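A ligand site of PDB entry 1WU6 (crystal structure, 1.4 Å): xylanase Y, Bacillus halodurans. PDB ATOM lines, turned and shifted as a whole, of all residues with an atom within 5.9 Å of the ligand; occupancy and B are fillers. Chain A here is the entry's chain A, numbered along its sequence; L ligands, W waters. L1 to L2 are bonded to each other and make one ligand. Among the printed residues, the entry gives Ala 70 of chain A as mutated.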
ATOM      1  N   ARG A  68     -17.346  19.262  11.132  1.00  0.00           N
ATOM      2  CA  ARG A  68     -16.024  19.738  10.729  1.00  0.00           C
ATOM      3  C   ARG A  68     -15.142  20.201  11.872  1.00  0.00           C
ATOM      4  O   ARG A  68     -15.633  20.703  12.885  1.00  0.00           O
ATOM      5  CB  ARG A  68     -16.197  20.858   9.696  1.00  0.00           C
ATOM      6  CG  ARG A  68     -17.028  20.406   8.513  1.00  0.00           C
ATOM      7  CD  ARG A  68     -17.234  21.460   7.457  1.00  0.00           C
ATOM      8  NE  ARG A  68     -17.777  20.825   6.262  1.00  0.00           N
ATOM      9  CZ  ARG A  68     -17.759  21.338   5.039  1.00  0.00           C
ATOM     10  NH1 ARG A  68     -17.218  22.539   4.818  1.00  0.00           N
ATOM     11  NH2 ARG A  68     -18.235  20.634   4.026  1.00  0.00           N
ATOM     12  N   THR A  69     -13.827  20.039  11.721  1.00  0.00           N
ATOM     13  CA  THR A  69     -12.934  20.451  12.795  1.00  0.00           C
ATOM     14  C   THR A  69     -13.008  21.957  13.040  1.00  0.00           C
ATOM     15  O   THR A  69     -12.810  22.405  14.164  1.00  0.00           O
ATOM     16  CB  THR A  69     -11.460  20.026  12.547  1.00  0.00           C
ATOM     17  OG1 THR A  69     -11.057  20.415  11.227  1.00  0.00           O
ATOM     18  CG2 THR A  69     -11.323  18.519  12.695  1.00  0.00           C
ATOM     19  N   ALA A  70     -13.291  22.733  11.997  1.00  0.00           N
ATOM     20  CA  ALA A  70     -13.410  24.178  12.202  1.00  0.00           C
ATOM     21  C   ALA A  70     -14.573  24.430  13.148  1.00  0.00           C
ATOM     22  O   ALA A  70     -14.471  25.246  14.065  1.00  0.00           O
ATOM     23  CB  ALA A  70     -13.645  24.884  10.866  1.00  0.00           C
ATOM     24  N   TYR A  74     -14.391  25.635  17.013  1.00  0.00           N
ATOM     25  CA  TYR A  74     -15.128  26.858  17.306  1.00  0.00           C
ATOM     26  C   TYR A  74     -15.987  26.628  18.541  1.00  0.00           C
ATOM     27  O   TYR A  74     -16.044  27.462  19.450  1.00  0.00           O
ATOM     28  CB  TYR A  74     -16.089  27.247  16.175  1.00  0.00           C
ATOM     29  CG  TYR A  74     -15.481  27.846  14.934  1.00  0.00           C
ATOM     30  CD1 TYR A  74     -14.179  28.357  14.926  1.00  0.00           C
ATOM     31  CD2 TYR A  74     -16.234  27.929  13.761  1.00  0.00           C
ATOM     32  CE1 TYR A  74     -13.653  28.934  13.775  1.00  0.00           C
ATOM     33  CE2 TYR A  74     -15.717  28.510  12.605  1.00  0.00           C
ATOM     34  CZ  TYR A  74     -14.422  29.006  12.622  1.00  0.00           C
ATOM     35  OH  TYR A  74     -13.913  29.581  11.476  1.00  0.00           O
ATOM     36  N   TRP A 112     -10.695  16.344   9.046  1.00  0.00           N
ATOM     37  CA  TRP A 112     -11.487  17.564   8.952  1.00  0.00           C
ATOM     38  C   TRP A 112     -13.000  17.451   8.835  1.00  0.00           C
ATOM     39  O   TRP A 112     -13.715  18.351   9.283  1.00  0.00           O
ATOM     40  CB  TRP A 112     -10.965  18.456   7.813  1.00  0.00           C
ATOM     41  CG  TRP A 112     -11.534  18.158   6.458  1.00  0.00           C
ATOM     42  CD1 TRP A 112     -11.082  17.233   5.555  1.00  0.00           C
ATOM     43  CD2 TRP A 112     -12.642  18.817   5.828  1.00  0.00           C
ATOM     44  NE1 TRP A 112     -11.844  17.280   4.413  1.00  0.00           N
ATOM     45  CE2 TRP A 112     -12.807  18.249   4.557  1.00  0.00           C
ATOM     46  CE3 TRP A 112     -13.504  19.849   6.233  1.00  0.00           C
ATOM     47  CZ2 TRP A 112     -13.800  18.656   3.665  1.00  0.00           C
ATOM     48  CZ3 TRP A 112     -14.500  20.259   5.350  1.00  0.00           C
ATOM     49  CH2 TRP A 112     -14.642  19.667   4.083  1.00  0.00           C
ATOM     50  N   SER A 122     -12.908  11.950   5.387  1.00  0.00           N
ATOM     51  CA  SER A 122     -11.583  12.232   4.850  1.00  0.00           C
ATOM     52  C   SER A 122     -10.541  11.974   5.921  1.00  0.00           C
ATOM     53  O   SER A 122     -10.850  11.997   7.110  1.00  0.00           O
ATOM     54  CB  SER A 122     -11.514  13.697   4.412  1.00  0.00           C
ATOM     55  OG  SER A 122     -10.200  14.082   4.059  1.00  0.00           O
ATOM     56  N   GLY A 124      -7.768  13.780   5.759  1.00  0.00           N
ATOM     57  CA  GLY A 124      -6.980  14.998   5.644  1.00  0.00           C
ATOM     58  C   GLY A 124      -7.450  15.978   6.700  1.00  0.00           C
ATOM     59  O   GLY A 124      -8.634  15.972   7.057  1.00  0.00           O
ATOM     60  N   PRO A 125      -6.550  16.815   7.238  1.00  0.00           N
ATOM     61  CA  PRO A 125      -6.911  17.789   8.268  1.00  0.00           C
ATOM     62  C   PRO A 125      -7.099  19.207   7.719  1.00  0.00           C
ATOM     63  O   PRO A 125      -6.846  19.470   6.545  1.00  0.00           O
ATOM     64  CB  PRO A 125      -5.737  17.706   9.224  1.00  0.00           C
ATOM     65  CG  PRO A 125      -4.593  17.622   8.258  1.00  0.00           C
ATOM     66  CD  PRO A 125      -5.090  16.634   7.191  1.00  0.00           C
ATOM     67  N   ALA A 126      -7.560  20.109   8.593  1.00  0.00           N
ATOM     68  CA  ALA A 126      -7.768  21.511   8.255  1.00  0.00           C
ATOM     69  C   ALA A 126      -7.040  22.336   9.317  1.00  0.00           C
ATOM     70  O   ALA A 126      -7.467  22.395  10.462  1.00  0.00           O
ATOM     71  CB  ALA A 126      -9.258  21.841   8.261  1.00  0.00           C
ATOM     72  N   PRO A 127      -5.926  22.988   8.934  1.00  0.00           N
ATOM     73  CA  PRO A 127      -5.141  23.808   9.861  1.00  0.00           C
ATOM     74  C   PRO A 127      -5.906  24.817  10.711  1.00  0.00           C
ATOM     75  O   PRO A 127      -5.523  25.062  11.860  1.00  0.00           O
ATOM     76  CB  PRO A 127      -4.119  24.479   8.946  1.00  0.00           C
ATOM     77  CG  PRO A 127      -3.892  23.439   7.902  1.00  0.00           C
ATOM     78  CD  PRO A 127      -5.295  22.951   7.609  1.00  0.00           C
ATOM     79  N   ASP A 128      -6.960  25.414  10.179  1.00  0.00           N
ATOM     80  CA  ASP A 128      -7.690  26.376  10.990  1.00  0.00           C
ATOM     81  C   ASP A 128      -8.380  25.686  12.166  1.00  0.00           C
ATOM     82  O   ASP A 128      -8.615  26.315  13.205  1.00  0.00           O
ATOM     83  CB  ASP A 128      -8.666  27.216  10.133  1.00  0.00           C
ATOM     84  CG  ASP A 128      -9.732  26.390   9.431  1.00  0.00           C
ATOM     85  OD1 ASP A 128      -9.421  25.299   8.904  1.00  0.00           O
ATOM     86  OD2 ASP A 128     -10.887  26.863   9.397  1.00  0.00           O
ATOM     87  N   GLY A 129      -8.665  24.395  12.030  1.00  0.00           N
ATOM     88  CA  GLY A 129      -9.271  23.657  13.118  1.00  0.00           C
ATOM     89  C   GLY A 129      -8.213  23.437  14.193  1.00  0.00           C
ATOM     90  O   GLY A 129      -8.433  23.731  15.365  1.00  0.00           O
ATOM     91  N   PHE A 187      -2.764  26.053   3.745  1.00  0.00           N
ATOM     92  CA  PHE A 187      -4.174  25.742   3.533  1.00  0.00           C
ATOM     93  C   PHE A 187      -4.394  24.299   4.021  1.00  0.00           C
ATOM     94  O   PHE A 187      -5.373  24.009   4.708  1.00  0.00           O
ATOM     95  CB  PHE A 187      -4.545  25.867   2.047  1.00  0.00           C
ATOM     96  CG  PHE A 187      -5.811  25.142   1.673  1.00  0.00           C
ATOM     97  CD1 PHE A 187      -7.011  25.448   2.296  1.00  0.00           C
ATOM     98  CD2 PHE A 187      -5.777  24.120   0.732  1.00  0.00           C
ATOM     99  CE1 PHE A 187      -8.180  24.746   1.972  1.00  0.00           C
ATOM    100  CE2 PHE A 187      -6.930  23.419   0.401  1.00  0.00           C
ATOM    101  CZ  PHE A 187      -8.130  23.726   1.024  1.00  0.00           C
ATOM    102  N   ILE A 188      -3.477  23.413   3.643  1.00  0.00           N
ATOM    103  CA  ILE A 188      -3.477  22.017   4.105  1.00  0.00           C
ATOM    104  C   ILE A 188      -2.011  21.606   4.162  1.00  0.00           C
ATOM    105  O   ILE A 188      -1.162  22.214   3.497  1.00  0.00           O
ATOM    106  CB  ILE A 188      -4.303  21.040   3.206  1.00  0.00           C
ATOM    107  CG1 ILE A 188      -3.856  21.108   1.744  1.00  0.00           C
ATOM    108  CG2 ILE A 188      -5.790  21.333   3.360  1.00  0.00           C
ATOM    109  CD1 ILE A 188      -4.604  20.133   0.839  1.00  0.00           C
ATOM    110  N   TYR A 198      -7.182  31.986   7.717  1.00  0.00           N
ATOM    111  CA  TYR A 198      -6.547  31.072   8.666  1.00  0.00           C
ATOM    112  C   TYR A 198      -5.483  31.771   9.513  1.00  0.00           C
ATOM    113  O   TYR A 198      -5.038  31.223  10.524  1.00  0.00           O
ATOM    114  CB  TYR A 198      -5.858  29.924   7.927  1.00  0.00           C
ATOM    115  CG  TYR A 198      -6.762  28.871   7.317  1.00  0.00           C
ATOM    116  CD1 TYR A 198      -8.130  29.095   7.136  1.00  0.00           C
ATOM    117  CD2 TYR A 198      -6.226  27.658   6.880  1.00  0.00           C
ATOM    118  CE1 TYR A 198      -8.943  28.122   6.542  1.00  0.00           C
ATOM    119  CE2 TYR A 198      -7.027  26.689   6.289  1.00  0.00           C
ATOM    120  CZ  TYR A 198      -8.380  26.930   6.119  1.00  0.00           C
ATOM    121  OH  TYR A 198      -9.165  25.972   5.508  1.00  0.00           O
ATOM    122  N   TYR A 244      -8.469  31.606  -0.894  1.00  0.00           N
ATOM    123  CA  TYR A 244      -7.165  30.943  -0.964  1.00  0.00           C
ATOM    124  C   TYR A 244      -6.196  31.925  -1.614  1.00  0.00           C
ATOM    125  O   TYR A 244      -6.576  32.670  -2.525  1.00  0.00           O
ATOM    126  CB  TYR A 244      -7.173  29.688  -1.851  1.00  0.00           C
ATOM    127  CG  TYR A 244      -7.989  28.491  -1.384  1.00  0.00           C
ATOM    128  CD1 TYR A 244      -8.741  28.528  -0.203  1.00  0.00           C
ATOM    129  CD2 TYR A 244      -8.038  27.343  -2.166  1.00  0.00           C
ATOM    130  CE1 TYR A 244      -9.529  27.440   0.169  1.00  0.00           C
ATOM    131  CE2 TYR A 244      -8.818  26.261  -1.804  1.00  0.00           C
ATOM    132  CZ  TYR A 244      -9.565  26.316  -0.639  1.00  0.00           C
ATOM    133  OH  TYR A 244     -10.376  25.243  -0.325  1.00  0.00           O
ATOM    134  N   TYR A 257     -11.593  29.461  -5.540  1.00  0.00           N
ATOM    135  CA  TYR A 257     -11.430  30.071  -4.227  1.00  0.00           C
ATOM    136  C   TYR A 257     -10.620  31.362  -4.226  1.00  0.00           C
ATOM    137  O   TYR A 257     -10.148  31.808  -3.181  1.00  0.00           O
ATOM    138  CB  TYR A 257     -10.771  29.063  -3.270  1.00  0.00           C
ATOM    139  CG  TYR A 257     -11.664  27.906  -2.901  1.00  0.00           C
ATOM    140  CD1 TYR A 257     -12.536  27.995  -1.815  1.00  0.00           C
ATOM    141  CD2 TYR A 257     -11.647  26.717  -3.634  1.00  0.00           C
ATOM    142  CE1 TYR A 257     -13.385  26.947  -1.478  1.00  0.00           C
ATOM    143  CE2 TYR A 257     -12.494  25.654  -3.314  1.00  0.00           C
ATOM    144  CZ  TYR A 257     -13.352  25.769  -2.232  1.00  0.00           C
ATOM    145  OH  TYR A 257     -14.192  24.727  -1.906  1.00  0.00           O
ATOM    146  N   ASP A 263     -14.964  31.914   3.240  1.00  0.00           N
ATOM    147  CA  ASP A 263     -13.751  31.916   4.058  1.00  0.00           C
ATOM    148  C   ASP A 263     -13.287  33.337   4.415  1.00  0.00           C
ATOM    149  O   ASP A 263     -12.970  33.630   5.569  1.00  0.00           O
ATOM    150  CB  ASP A 263     -12.605  31.220   3.327  1.00  0.00           C
ATOM    151  CG  ASP A 263     -12.656  29.708   3.430  1.00  0.00           C
ATOM    152  OD1 ASP A 263     -13.755  29.137   3.556  1.00  0.00           O
ATOM    153  OD2 ASP A 263     -11.567  29.083   3.359  1.00  0.00           O
ATOM    154  N   ARG A 266     -14.001  35.935   7.562  1.00  0.00           N
ATOM    155  CA  ARG A 266     -13.310  35.867   8.842  1.00  0.00           C
ATOM    156  C   ARG A 266     -12.115  36.805   8.982  1.00  0.00           C
ATOM    157  O   ARG A 266     -11.707  37.124  10.103  1.00  0.00           O
ATOM    158  CB  ARG A 266     -12.911  34.421   9.130  1.00  0.00           C
ATOM    159  CG  ARG A 266     -14.123  33.508   9.255  1.00  0.00           C
ATOM    160  CD  ARG A 266     -13.759  32.043   9.358  1.00  0.00           C
ATOM    161  NE  ARG A 266     -13.108  31.550   8.142  1.00  0.00           N
ATOM    162  CZ  ARG A 266     -13.011  30.262   7.819  1.00  0.00           C
ATOM    163  NH1 ARG A 266     -13.530  29.341   8.622  1.00  0.00           N
ATOM    164  NH2 ARG A 266     -12.392  29.893   6.705  1.00  0.00           N
ATOM    165  N   TYR A 359     -25.536  27.254  10.040  1.00  0.00           N
ATOM    166  CA  TYR A 359     -24.321  26.921  10.785  1.00  0.00           C
ATOM    167  C   TYR A 359     -23.186  27.942  10.718  1.00  0.00           C
ATOM    168  O   TYR A 359     -22.769  28.484  11.743  1.00  0.00           O
ATOM    169  CB  TYR A 359     -23.819  25.539  10.328  1.00  0.00           C
ATOM    170  CG  TYR A 359     -22.362  25.259  10.616  1.00  0.00           C
ATOM    171  CD1 TYR A 359     -21.927  24.905  11.892  1.00  0.00           C
ATOM    172  CD2 TYR A 359     -21.422  25.325   9.590  1.00  0.00           C
ATOM    173  CE1 TYR A 359     -20.574  24.606  12.126  1.00  0.00           C
ATOM    174  CE2 TYR A 359     -20.086  25.034   9.817  1.00  0.00           C
ATOM    175  CZ  TYR A 359     -19.676  24.671  11.086  1.00  0.00           C
ATOM    176  OH  TYR A 359     -18.342  24.377  11.290  1.00  0.00           O
ATOM    177  N   TYR A 360     -22.668  28.194   9.520  1.00  0.00           N
ATOM    178  CA  TYR A 360     -21.547  29.119   9.369  1.00  0.00           C
ATOM    179  C   TYR A 360     -21.875  30.521   9.838  1.00  0.00           C
ATOM    180  O   TYR A 360     -21.092  31.150  10.552  1.00  0.00           O
ATOM    181  CB  TYR A 360     -21.084  29.143   7.907  1.00  0.00           C
ATOM    182  CG  TYR A 360     -19.748  29.813   7.698  1.00  0.00           C
ATOM    183  CD1 TYR A 360     -18.589  29.302   8.272  1.00  0.00           C
ATOM    184  CD2 TYR A 360     -19.648  30.956   6.913  1.00  0.00           C
ATOM    185  CE1 TYR A 360     -17.349  29.899   8.066  1.00  0.00           C
ATOM    186  CE2 TYR A 360     -18.407  31.575   6.699  1.00  0.00           C
ATOM    187  CZ  TYR A 360     -17.271  31.041   7.273  1.00  0.00           C
ATOM    188  OH  TYR A 360     -16.049  31.635   7.050  1.00  0.00           O
HETATM  189  O1  LIG L   1     -15.459  26.562   6.675  1.00  0.00           O
HETATM  190  C1  LIG L   1     -14.362  25.940   6.102  1.00  0.00           C
HETATM  191  C2  LIG L   1     -13.352  25.575   7.186  1.00  0.00           C
HETATM  192  C3  LIG L   1     -12.186  24.774   6.599  1.00  0.00           C
HETATM  193  C4  LIG L   1     -12.603  23.690   5.572  1.00  0.00           C
HETATM  194  C5  LIG L   1     -13.772  24.137   4.681  1.00  0.00           C
HETATM  195  O2  LIG L   1     -12.849  26.765   7.771  1.00  0.00           O
HETATM  196  O3  LIG L   1     -11.490  24.142   7.663  1.00  0.00           O
HETATM  197  O4  LIG L   1     -11.475  23.435   4.715  1.00  0.00           O
HETATM  198  O5  LIG L   1     -14.812  24.746   5.458  1.00  0.00           O
HETATM  199  C1  LG2 L   2     -11.259  22.145   4.279  1.00  0.00           C
HETATM  200  C2  LG2 L   2     -11.143  22.154   2.740  1.00  0.00           C
HETATM  201  C3  LG2 L   2     -10.719  20.771   2.221  1.00  0.00           C
HETATM  202  C4  LG2 L   2      -9.430  20.333   2.917  1.00  0.00           C
HETATM  203  C5  LG2 L   2      -9.637  20.372   4.440  1.00  0.00           C
HETATM  204  O1  LG2 L   2     -12.382  22.513   2.157  1.00  0.00           O
HETATM  205  O2  LG2 L   2     -10.516  20.833   0.819  1.00  0.00           O
HETATM  206  O3  LG2 L   2      -9.082  19.021   2.514  1.00  0.00           O
HETATM  207  O4  LG2 L   2     -10.019  21.705   4.857  1.00  0.00           O
HETATM  208  O   HOH W   1     -16.773  24.866   9.081  1.00  0.00           O
HETATM  209  O   HOH W   2     -10.541  22.841  -1.531  1.00  0.00           O
HETATM  210  O   HOH W   3      -8.057  23.559   5.415  1.00  0.00           O
HETATM  211  O   HOH W   4     -11.754  18.383  -0.209  1.00  0.00           O
HETATM  212  O   HOH W   5      -8.073  19.022  -0.264  1.00  0.00           O
HETATM  213  O   HOH W   6     -12.235  25.213   1.642  1.00  0.00           O
HETATM  214  O   HOH W   7      -7.069  18.014   4.185  1.00  0.00           O
HETATM  215  O   HOH W   8     -14.567  21.222   0.830  1.00  0.00           O
HETATM  216  O   HOH W   9     -15.796  28.938   5.180  1.00  0.00           O
HETATM  217  O   HOH W  10     -15.721  27.128   9.616  1.00  0.00           O
HETATM  218  O   HOH W  11     -11.295  26.513   3.756  1.00  0.00           O
HETATM  219  O   HOH W  12     -12.647  21.956   9.211  1.00  0.00           O
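O2 of LIG L1 lies within hydrogen-bond range of OD2 of Asp 128 (2.6 Å). The guanidinium group (NH1) of Arg 266 lies within hydrogen-bond range of an oxygen (O2) of LIG L1 (2.8 Å). NH1 of Arg 68 is in hydrogen-bond range of O5 of LIG L1, 3.3 Å away.
OD2 of Asp 128 lies within salt-bridge range of NH1 of Arg 266 (3.7 Å). The side-chain carboxylate (OD1) of Asp 128 sits close to the side-chain hydroxyl (OH) of Tyr 198 (3.5 Å). NE of Arg 266 is in hydrogen-bond range of OH of Tyr 360 (3.1 Å). NH2 of Arg 266 is in salt-bridge range of OD1 of Asp 263 (3.5 Å). The side-chain hydroxyl of Tyr 74 sits at hydrogen-bond distance from the guanidinium group of Arg 266, 2.9 Å away. The backbone carbonyl oxygen (O) of Trp 112 lies within hydrogen-bond range of the backbone NH (N) of Thr 69, at 3.0 Å. The backbone NH of Trp 112 is in hydrogen-bond range of the backbone carbonyl oxygen of Gly 124, 2.9 Å away.
Residues that only touch the ligand: Ala 126 (3.3 Å), Tyr 198 (3.4 Å), Trp 112 (3.5 Å), Pro 125 (3.6 Å), Ala 70 (3.7 Å), Phe 187 (3.8 Å) and Ile 188 (3.8 Å). Hydrophobic or aromatic side chains that line the ligand: Ala 70, Trp 112, Ala 126, Phe 187 and Ile 188. Within 4 Å of the ligand: Arg 68, Ala 70, Trp 112, Pro 125, Ala 126, Asp 128, Phe 187, Ile 188, Tyr 198 and Arg 266. Along chain A the residues within 4 Å of the ligand span positions 68 to 266. The nearest printed residue that does not touch the ligand is Tyr 360 (4.1 Å).
Water W6 lies within hydrogen-bond range of OH of Tyr 244 (2.7 Å) and O1 of LG2 L2 (2.8 Å). Water W3 lies within hydrogen-bond range of the side-chain hydroxyl of Tyr 198 (2.7 Å), an oxygen (O4) of LG2 L2 (2.8 Å) and the backbone carbonyl oxygen of Phe 187 (2.8 Å). Water W9 lies within hydrogen-bond range of OD1 of Asp 263 (2.6 Å), O1 of LIG L1 (2.8 Å) and OH of Tyr 360 (3.3 Å). Water W12 lies within hydrogen-bond range of an oxygen (O3) of LIG L1 (2.9 Å), the backbone NH (N) of Ala 70 (3.0 Å) and the side-chain hydroxyl (OG1) of Thr 69 (3.0 Å). Water W2 bridges the side-chain hydroxyl (OH) of Tyr 244 (2.7 Å) and an oxygen (O2) of LG2 L2 (3.1 Å). Water W1 bridges OH of Tyr 359 (2.8 Å) and O1 of LIG L1 (3.2 Å).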
